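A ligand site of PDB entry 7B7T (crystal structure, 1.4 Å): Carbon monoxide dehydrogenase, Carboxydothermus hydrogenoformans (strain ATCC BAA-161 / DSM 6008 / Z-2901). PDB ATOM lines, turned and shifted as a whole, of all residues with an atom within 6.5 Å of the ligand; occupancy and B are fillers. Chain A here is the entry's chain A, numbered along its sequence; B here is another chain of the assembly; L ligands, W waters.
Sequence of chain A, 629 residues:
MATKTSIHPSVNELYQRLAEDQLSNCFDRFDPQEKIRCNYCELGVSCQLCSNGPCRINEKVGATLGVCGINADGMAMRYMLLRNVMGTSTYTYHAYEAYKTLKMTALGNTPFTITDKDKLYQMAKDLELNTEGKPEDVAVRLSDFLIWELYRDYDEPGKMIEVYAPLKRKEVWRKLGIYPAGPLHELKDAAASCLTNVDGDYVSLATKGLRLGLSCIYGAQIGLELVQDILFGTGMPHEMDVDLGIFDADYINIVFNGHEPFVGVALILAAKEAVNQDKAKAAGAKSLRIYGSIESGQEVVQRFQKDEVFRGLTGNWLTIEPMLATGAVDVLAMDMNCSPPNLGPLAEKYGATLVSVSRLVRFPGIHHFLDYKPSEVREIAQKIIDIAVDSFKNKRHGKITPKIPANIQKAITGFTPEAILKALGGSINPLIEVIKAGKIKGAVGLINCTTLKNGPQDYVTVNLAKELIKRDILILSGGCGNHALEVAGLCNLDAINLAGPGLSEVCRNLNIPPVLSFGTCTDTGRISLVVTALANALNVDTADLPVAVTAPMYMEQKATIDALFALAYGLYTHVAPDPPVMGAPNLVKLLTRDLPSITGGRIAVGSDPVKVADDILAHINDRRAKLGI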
ATOM      1  N   SER A  46       4.758  32.453   0.695  1.00  0.00           N
ATOM      2  CA  SER A  46       5.467  32.452   1.961  1.00  0.00           C
ATOM      3  C   SER A  46       4.493  31.975   3.021  1.00  0.00           C
ATOM      4  O   SER A  46       3.275  32.057   2.863  1.00  0.00           O
ATOM      5  CB  SER A  46       5.937  33.852   2.344  1.00  0.00           C
ATOM      6  OG  SER A  46       4.817  34.710   2.632  1.00  0.00           O
ATOM      7  N   CYS A  47       5.056  31.536   4.139  1.00  0.00           N
ATOM      8  CA  CYS A  47       4.282  31.019   5.260  1.00  0.00           C
ATOM      9  C   CYS A  47       5.003  31.311   6.566  1.00  0.00           C
ATOM     10  O   CYS A  47       6.219  31.109   6.671  1.00  0.00           O
ATOM     11  CB  CYS A  47       4.065  29.518   5.107  1.00  0.00           C
ATOM     12  SG  CYS A  47       2.918  28.835   6.357  1.00  0.00           S
ATOM     13  N   GLN A  48       4.252  31.749   7.565  1.00  0.00           N
ATOM     14  CA  GLN A  48       4.780  32.060   8.880  1.00  0.00           C
ATOM     15  C   GLN A  48       3.978  31.349   9.957  1.00  0.00           C
ATOM     16  O   GLN A  48       3.895  31.830  11.088  1.00  0.00           O
ATOM     17  CB  GLN A  48       4.814  33.570   9.120  1.00  0.00           C
ATOM     18  CG  GLN A  48       5.495  34.344   8.045  1.00  0.00           C
ATOM     19  CD  GLN A  48       4.642  34.615   6.784  1.00  0.00           C
ATOM     20  OE1 GLN A  48       3.422  34.660   6.838  1.00  0.00           O
ATOM     21  NE2 GLN A  48       5.315  34.731   5.635  1.00  0.00           N
ATOM     22  N   LEU A  49       3.365  30.218   9.657  1.00  0.00           N
ATOM     23  CA  LEU A  49       2.410  29.647  10.614  1.00  0.00           C
ATOM     24  C   LEU A  49       3.002  28.757  11.683  1.00  0.00           C
ATOM     25  O   LEU A  49       2.271  28.426  12.611  1.00  0.00           O
ATOM     26  CB  LEU A  49       1.295  28.887   9.883  1.00  0.00           C
ATOM     27  CG  LEU A  49       0.414  29.720   8.966  1.00  0.00           C
ATOM     28  CD1 LEU A  49      -0.748  28.850   8.395  1.00  0.00           C
ATOM     29  CD2 LEU A  49      -0.154  30.907   9.677  1.00  0.00           C
ATOM     30  N   CYS A  50       4.261  28.336  11.591  1.00  0.00           N
ATOM     31  CA  CYS A  50       4.822  27.517  12.674  1.00  0.00           C
ATOM     32  C   CYS A  50       6.314  27.754  12.826  1.00  0.00           C
ATOM     33  O   CYS A  50       6.958  28.467  12.032  1.00  0.00           O
ATOM     34  CB  CYS A  50       4.517  26.026  12.469  1.00  0.00           C
ATOM     35  SG  CYS A  50       5.714  25.187  11.411  1.00  0.00           S
ATOM     36  N   SER A  51       6.877  27.171  13.911  1.00  0.00           N
ATOM     37  CA  SER A  51       8.257  27.491  14.248  1.00  0.00           C
ATOM     38  C   SER A  51       9.278  26.854  13.325  1.00  0.00           C
ATOM     39  O   SER A  51      10.446  27.279  13.364  1.00  0.00           O
ATOM     40  CB  SER A  51       8.575  27.057  15.669  1.00  0.00           C
ATOM     41  OG  SER A  51       8.727  25.646  15.758  1.00  0.00           O
ATOM     42  N   ASN A  52       8.903  25.854  12.525  1.00  0.00           N
ATOM     43  CA  ASN A  52       9.842  25.327  11.542  1.00  0.00           C
ATOM     44  C   ASN A  52      10.090  26.311  10.417  1.00  0.00           C
ATOM     45  O   ASN A  52      11.058  26.144   9.665  1.00  0.00           O
ATOM     46  CB  ASN A  52       9.377  23.985  10.959  1.00  0.00           C
ATOM     47  CG  ASN A  52       9.873  22.772  11.759  1.00  0.00           C
ATOM     48  OD1 ASN A  52      10.994  22.720  12.239  1.00  0.00           O
ATOM     49  ND2 ASN A  52       9.030  21.755  11.829  1.00  0.00           N
ATOM     50  N   GLY A  53       9.196  27.285  10.250  1.00  0.00           N
ATOM     51  CA  GLY A  53       9.342  28.338   9.272  1.00  0.00           C
ATOM     52  C   GLY A  53      10.231  29.448   9.788  1.00  0.00           C
ATOM     53  O   GLY A  53      10.995  29.258  10.733  1.00  0.00           O
ATOM     54  N   PRO A  54      10.098  30.627   9.204  1.00  0.00           N
ATOM     55  CA  PRO A  54       9.198  30.952   8.096  1.00  0.00           C
ATOM     56  C   PRO A  54       9.651  30.256   6.813  1.00  0.00           C
ATOM     57  O   PRO A  54      10.848  30.004   6.637  1.00  0.00           O
ATOM     58  CB  PRO A  54       9.327  32.455   7.995  1.00  0.00           C
ATOM     59  CG  PRO A  54      10.699  32.748   8.507  1.00  0.00           C
ATOM     60  CD  PRO A  54      10.962  31.753   9.582  1.00  0.00           C
ATOM     61  N   CYS A  55       8.729  29.932   5.933  1.00  0.00           N
ATOM     62  CA  CYS A  55       8.997  29.186   4.715  1.00  0.00           C
ATOM     63  C   CYS A  55       8.639  29.996   3.476  1.00  0.00           C
ATOM     64  O   CYS A  55       7.837  30.936   3.523  1.00  0.00           O
ATOM     65  CB  CYS A  55       8.208  27.874   4.716  1.00  0.00           C
ATOM     66  SG  CYS A  55       8.738  26.694   5.934  1.00  0.00           S
ATOM     67  N   ARG A  56       9.259  29.607   2.368  1.00  0.00           N
ATOM     68  CA  ARG A  56       9.086  30.187   1.054  1.00  0.00           C
ATOM     69  C   ARG A  56       9.129  29.066   0.034  1.00  0.00           C
ATOM     70  O   ARG A  56       9.875  28.104   0.192  1.00  0.00           O
ATOM     71  CB  ARG A  56      10.253  31.141   0.740  1.00  0.00           C
ATOM     72  CG  ARG A  56      10.150  32.443   1.497  1.00  0.00           C
ATOM     73  CD  ARG A  56      11.455  33.193   1.452  1.00  0.00           C
ATOM     74  NE  ARG A  56      11.243  34.589   1.721  1.00  0.00           N
ATOM     75  CZ  ARG A  56      12.175  35.532   1.608  1.00  0.00           C
ATOM     76  NH1 ARG A  56      13.414  35.194   1.368  1.00  0.00           N
ATOM     77  NH2 ARG A  56      11.850  36.808   1.798  1.00  0.00           N
ATOM     78  N   LEU A  65       8.641  22.636  -1.193  1.00  0.00           N
ATOM     79  CA  LEU A  65       7.625  22.469  -0.176  1.00  0.00           C
ATOM     80  C   LEU A  65       8.085  23.140   1.115  1.00  0.00           C
ATOM     81  O   LEU A  65       9.285  23.326   1.349  1.00  0.00           O
ATOM     82  CB  LEU A  65       7.424  20.978   0.113  1.00  0.00           C
ATOM     83  CG  LEU A  65       7.045  20.088  -1.061  1.00  0.00           C
ATOM     84  CD1 LEU A  65       6.997  18.601  -0.618  1.00  0.00           C
ATOM     85  CD2 LEU A  65       5.704  20.489  -1.714  1.00  0.00           C
ATOM     86  N   GLY A  66       7.141  23.526   1.956  1.00  0.00           N
ATOM     87  CA  GLY A  66       7.461  23.932   3.310  1.00  0.00           C
ATOM     88  C   GLY A  66       8.100  22.791   4.078  1.00  0.00           C
ATOM     89  O   GLY A  66       8.081  21.634   3.678  1.00  0.00           O
ATOM     90  N   VAL A  67       8.666  23.122   5.235  1.00  0.00           N
ATOM     91  CA  VAL A  67       9.283  22.081   6.050  1.00  0.00           C
ATOM     92  C   VAL A  67       8.286  20.962   6.340  1.00  0.00           C
ATOM     93  O   VAL A  67       8.629  19.779   6.294  1.00  0.00           O
ATOM     94  CB  VAL A  67       9.913  22.658   7.340  1.00  0.00           C
ATOM     95  CG1 VAL A  67      10.503  21.532   8.199  1.00  0.00           C
ATOM     96  CG2 VAL A  67      10.991  23.722   7.017  1.00  0.00           C
ATOM     97  N   CYS A  68       7.049  21.328   6.664  1.00  0.00           N
ATOM     98  CA  CYS A  68       5.996  20.376   6.976  1.00  0.00           C
ATOM     99  C   CYS A  68       5.578  19.521   5.788  1.00  0.00           C
ATOM    100  O   CYS A  68       4.914  18.502   5.986  1.00  0.00           O
ATOM    101  CB  CYS A  68       4.763  21.100   7.485  1.00  0.00           C
ATOM    102  SG  CYS A  68       4.102  22.303   6.270  1.00  0.00           S
ATOM    103  N   GLY A  69       5.884  19.936   4.558  1.00  0.00           N
ATOM    104  CA  GLY A  69       5.519  19.215   3.350  1.00  0.00           C
ATOM    105  C   GLY A  69       4.435  19.888   2.526  1.00  0.00           C
ATOM    106  O   GLY A  69       4.082  19.353   1.481  1.00  0.00           O
ATOM    107  N   ILE A  70       3.922  21.040   2.929  1.00  0.00           N
ATOM    108  CA  ILE A  70       2.833  21.652   2.176  1.00  0.00           C
ATOM    109  C   ILE A  70       3.380  22.264   0.877  1.00  0.00           C
ATOM    110  O   ILE A  70       4.527  22.754   0.807  1.00  0.00           O
ATOM    111  CB  ILE A  70       2.094  22.696   3.027  1.00  0.00           C
ATOM    112  CG1 ILE A  70       0.715  23.007   2.429  1.00  0.00           C
ATOM    113  CG2 ILE A  70       2.918  23.980   3.191  1.00  0.00           C
ATOM    114  CD1 ILE A  70      -0.201  23.842   3.354  1.00  0.00           C
ATOM    115  N   MET A  75      -0.411  26.235   0.548  1.00  0.00           N
ATOM    116  CA  MET A  75       0.067  27.368   1.334  1.00  0.00           C
ATOM    117  C   MET A  75      -0.747  28.625   1.057  1.00  0.00           C
ATOM    118  O   MET A  75      -1.205  29.296   1.991  1.00  0.00           O
ATOM    119  CB  MET A  75       1.559  27.594   1.011  1.00  0.00           C
ATOM    120  CG  MET A  75       2.205  28.712   1.750  1.00  0.00           C
ATOM    121  SD  MET A  75       3.969  28.938   1.286  1.00  0.00           S
ATOM    122  CE  MET A  75       4.666  27.407   1.916  1.00  0.00           C
ATOM    123  N   ARG A  78      -4.480  28.269   2.154  1.00  0.00           N
ATOM    124  CA  ARG A  78      -4.632  28.228   3.596  1.00  0.00           C
ATOM    125  C   ARG A  78      -4.580  29.633   4.184  1.00  0.00           C
ATOM    126  O   ARG A  78      -5.370  29.961   5.070  1.00  0.00           O
ATOM    127  CB  ARG A  78      -3.577  27.313   4.191  1.00  0.00           C
ATOM    128  CG  ARG A  78      -3.636  27.231   5.710  1.00  0.00           C
ATOM    129  CD  ARG A  78      -2.695  26.153   6.234  1.00  0.00           C
ATOM    130  NE  ARG A  78      -1.320  26.473   5.903  1.00  0.00           N
ATOM    131  CZ  ARG A  78      -0.291  25.725   6.244  1.00  0.00           C
ATOM    132  NH1 ARG A  78      -0.480  24.601   6.934  1.00  0.00           N
ATOM    133  NH2 ARG A  78       0.931  26.142   5.929  1.00  0.00           N
ATOM    134  N   CYS A 194      -6.617  25.426   9.379  1.00  0.00           N
ATOM    135  CA  CYS A 194      -5.423  26.141   8.957  1.00  0.00           C
ATOM    136  C   CYS A 194      -4.226  25.911   9.860  1.00  0.00           C
ATOM    137  O   CYS A 194      -3.128  26.341   9.519  1.00  0.00           O
ATOM    138  CB  CYS A 194      -5.722  27.647   8.915  1.00  0.00           C
ATOM    139  SG  CYS A 194      -6.889  28.127   7.582  1.00  0.00           S
ATOM    140  N   LEU A 195      -4.407  25.294  11.028  1.00  0.00           N
ATOM    141  CA  LEU A 195      -3.258  24.971  11.856  1.00  0.00           C
ATOM    142  C   LEU A 195      -2.323  24.051  11.094  1.00  0.00           C
ATOM    143  O   LEU A 195      -2.744  23.239  10.277  1.00  0.00           O
ATOM    144  CB  LEU A 195      -3.708  24.337  13.178  1.00  0.00           C
ATOM    145  CG  LEU A 195      -2.659  24.211  14.264  1.00  0.00           C
ATOM    146  CD1 LEU A 195      -2.847  25.321  15.295  1.00  0.00           C
ATOM    147  CD2 LEU A 195      -2.785  22.874  14.905  1.00  0.00           C
ATOM    148  N   THR A 196      -1.025  24.201  11.363  1.00  0.00           N
ATOM    149  CA  THR A 196      -0.045  23.364  10.710  1.00  0.00           C
ATOM    150  C   THR A 196      -0.412  21.889  10.824  1.00  0.00           C
ATOM    151  O   THR A 196      -0.840  21.409  11.867  1.00  0.00           O
ATOM    152  CB  THR A 196       1.318  23.646  11.370  1.00  0.00           C
ATOM    153  OG1 THR A 196       1.611  25.057  11.240  1.00  0.00           O
ATOM    154  CG2 THR A 196       2.417  22.797  10.716  1.00  0.00           C
ATOM    155  N   ASN A 197      -0.211  21.172   9.732  1.00  0.00           N
ATOM    156  CA  ASN A 197      -0.406  19.724   9.690  1.00  0.00           C
ATOM    157  C   ASN A 197      -1.850  19.320   9.930  1.00  0.00           C
ATOM    158  O   ASN A 197      -2.123  18.267  10.498  1.00  0.00           O
ATOM    159  CB  ASN A 197       0.545  19.001  10.650  1.00  0.00           C
ATOM    160  CG  ASN A 197       2.003  19.114  10.193  1.00  0.00           C
ATOM    161  OD1 ASN A 197       2.284  19.247   8.986  1.00  0.00           O
ATOM    162  ND2 ASN A 197       2.913  19.126  11.138  1.00  0.00           N
ATOM    163  N   GLN B  33      14.915  25.511   3.137  1.00  0.00           N
ATOM    164  CA  GLN B  33      14.256  26.687   3.707  1.00  0.00           C
ATOM    165  C   GLN B  33      15.257  27.546   4.467  1.00  0.00           C
ATOM    166  O   GLN B  33      15.186  28.775   4.428  1.00  0.00           O
ATOM    167  CB  GLN B  33      13.113  26.251   4.638  1.00  0.00           C
ATOM    168  CG  GLN B  33      11.952  25.625   3.919  1.00  0.00           C
ATOM    169  CD  GLN B  33      11.257  26.590   2.992  1.00  0.00           C
ATOM    170  OE1 GLN B  33      11.376  27.787   3.136  1.00  0.00           O
ATOM    171  NE2 GLN B  33      10.523  26.069   2.027  1.00  0.00           N
ATOM    172  N   ARG B  37      15.760  31.945   4.341  1.00  0.00           N
ATOM    173  CA  ARG B  37      14.926  32.446   5.432  1.00  0.00           C
ATOM    174  C   ARG B  37      14.815  33.960   5.384  1.00  0.00           C
ATOM    175  O   ARG B  37      15.808  34.687   5.235  1.00  0.00           O
ATOM    176  CB  ARG B  37      15.512  32.062   6.791  1.00  0.00           C
ATOM    177  CG  ARG B  37      15.686  30.598   7.032  1.00  0.00           C
ATOM    178  CD  ARG B  37      14.402  29.963   7.440  1.00  0.00           C
ATOM    179  NE  ARG B  37      14.555  28.564   7.846  1.00  0.00           N
ATOM    180  CZ  ARG B  37      13.544  27.724   8.035  1.00  0.00           C
ATOM    181  NH1 ARG B  37      13.751  26.479   8.446  1.00  0.00           N
ATOM    182  NH2 ARG B  37      12.314  28.124   7.825  1.00  0.00           N
ATOM    183  N   MET B 555       6.078  24.325  18.387  1.00  0.00           N
ATOM    184  CA  MET B 555       5.900  24.269  16.945  1.00  0.00           C
ATOM    185  C   MET B 555       4.684  25.053  16.473  1.00  0.00           C
ATOM    186  O   MET B 555       4.795  25.949  15.642  1.00  0.00           O
ATOM    187  CB  MET B 555       5.805  22.812  16.461  1.00  0.00           C
ATOM    188  CG  MET B 555       6.087  22.621  14.967  1.00  0.00           C
ATOM    189  SD  MET B 555       4.664  22.770  13.891  1.00  0.00           S
ATOM    190  CE  MET B 555       3.756  21.280  14.300  1.00  0.00           C
HETATM  191 FE1  LIG L   1       6.744  26.248   6.996  1.00  0.00          FE
HETATM  192 FE2  LIG L   1       5.340  25.819   9.255  1.00  0.00          FE
HETATM  193 FE3  LIG L   1       4.694  24.408   6.991  1.00  0.00          FE
HETATM  194 FE4  LIG L   1       4.198  27.120   7.172  1.00  0.00          FE
HETATM  195  S1  LIG L   1       3.191  25.497   8.407  1.00  0.00           S
HETATM  196  S2  LIG L   1       5.107  25.959   5.385  1.00  0.00           S
HETATM  197  S3  LIG L   1       5.956  27.858   8.455  1.00  0.00           S
HETATM  198  S4  LIG L   1       6.687  24.303   8.152  1.00  0.00           S
HETATM  199  O   HOH W   1       6.333  22.000  10.734  1.00  0.00           O
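An iron atom (FE4) of the ligand is bound by the side-chain sulfur (SG) of Cys 47 (2.3 Å). The side-chain hydroxyl (OG1) of Thr 196 sits close to a sulfur (S1) of the ligand (3.3 Å). SG of Cys 50 is bound to FE2 of the ligand, 2.3 Å away. The guanidinium group of Arg 78 sits close to a sulfur (S1) of the ligand (3.4 Å). The backbone NH (N) of Cys 68 sits close to a sulfur (S4) of the ligand, 3.3 Å away. The backbone NH (N) of Cys 50 lies close to a sulfur (S3) of the ligand (3.6 Å). The side-chain sulfur (SG) of Cys 55 binds an iron atom (FE1) of the ligand (2.3 Å). A sulfur (S3) of the ligand lies close to the backbone NH (N) of Leu 49 (3.7 Å). S3 of the ligand sits close to N of Gly 53, at 3.7 Å. A sulfur (S4) of the ligand sits close to the backbone NH of Val 67 (3.7 Å). An iron atom (FE3) of the ligand is bound by the side-chain sulfur of Cys 68, 2.3 Å away.
The guanidinium group (NH2) of Arg 37 of chain B lies close to the backbone carbonyl oxygen (O) of Gly 53, 3.4 Å away. The side-chain sulfur (SG) of Cys 194 sits at hydrogen-bond distance from the backbone carbonyl oxygen (O) of Arg 78. The backbone NH (N) of Leu 49 sits close to the side-chain sulfur (SG) of Cys 47 (3.6 Å). The backbone NH (N) of Ile 70 sits close to the side-chain sulfur (SG) of Cys 68. The side-chain sulfur of Met 75 sits close to the backbone NH of Ser 46, 3.7 Å away. NH1 of Arg 37 of chain B sits at hydrogen-bond distance from O of Asn 52 (3.0 Å). The side-chain sulfur (SG) of Cys 50 sits close to the side-chain sulfur (SD) of Met 555 of chain B (3.6 Å). SG of Cys 50 sits close to N of Asn 52 (3.4 Å).
CB of Asn 52 touches S4 of the ligand (3.9 Å). Gly 66 touches the ligand (CA to S2, 3.7 Å). CG2 of Ile 70 touches S2 of the ligand, at 3.7 Å. Met 75 touches the ligand (CE to S2, 3.8 Å). Hydrophobic or aromatic side chains that line the ligand: Val 67, Ile 70 and Met 75. 13 residues have an atom within 4 Å of the ligand: Cys 47, Leu 49, Cys 50, Asn 52, Gly 53, Cys 55, Gly 66, Val 67, Cys 68, Ile 70, Met 75, Arg 78 and Thr 196. The nearest printed residue that does not touch the ligand is Gln 48 (4.3 Å).
Water W1 lies within hydrogen-bond range of ND2 of Asn 52 (2.9 Å), S4 of the ligand (3.5 Å) and SD of Met 555 of chain B (3.7 Å).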
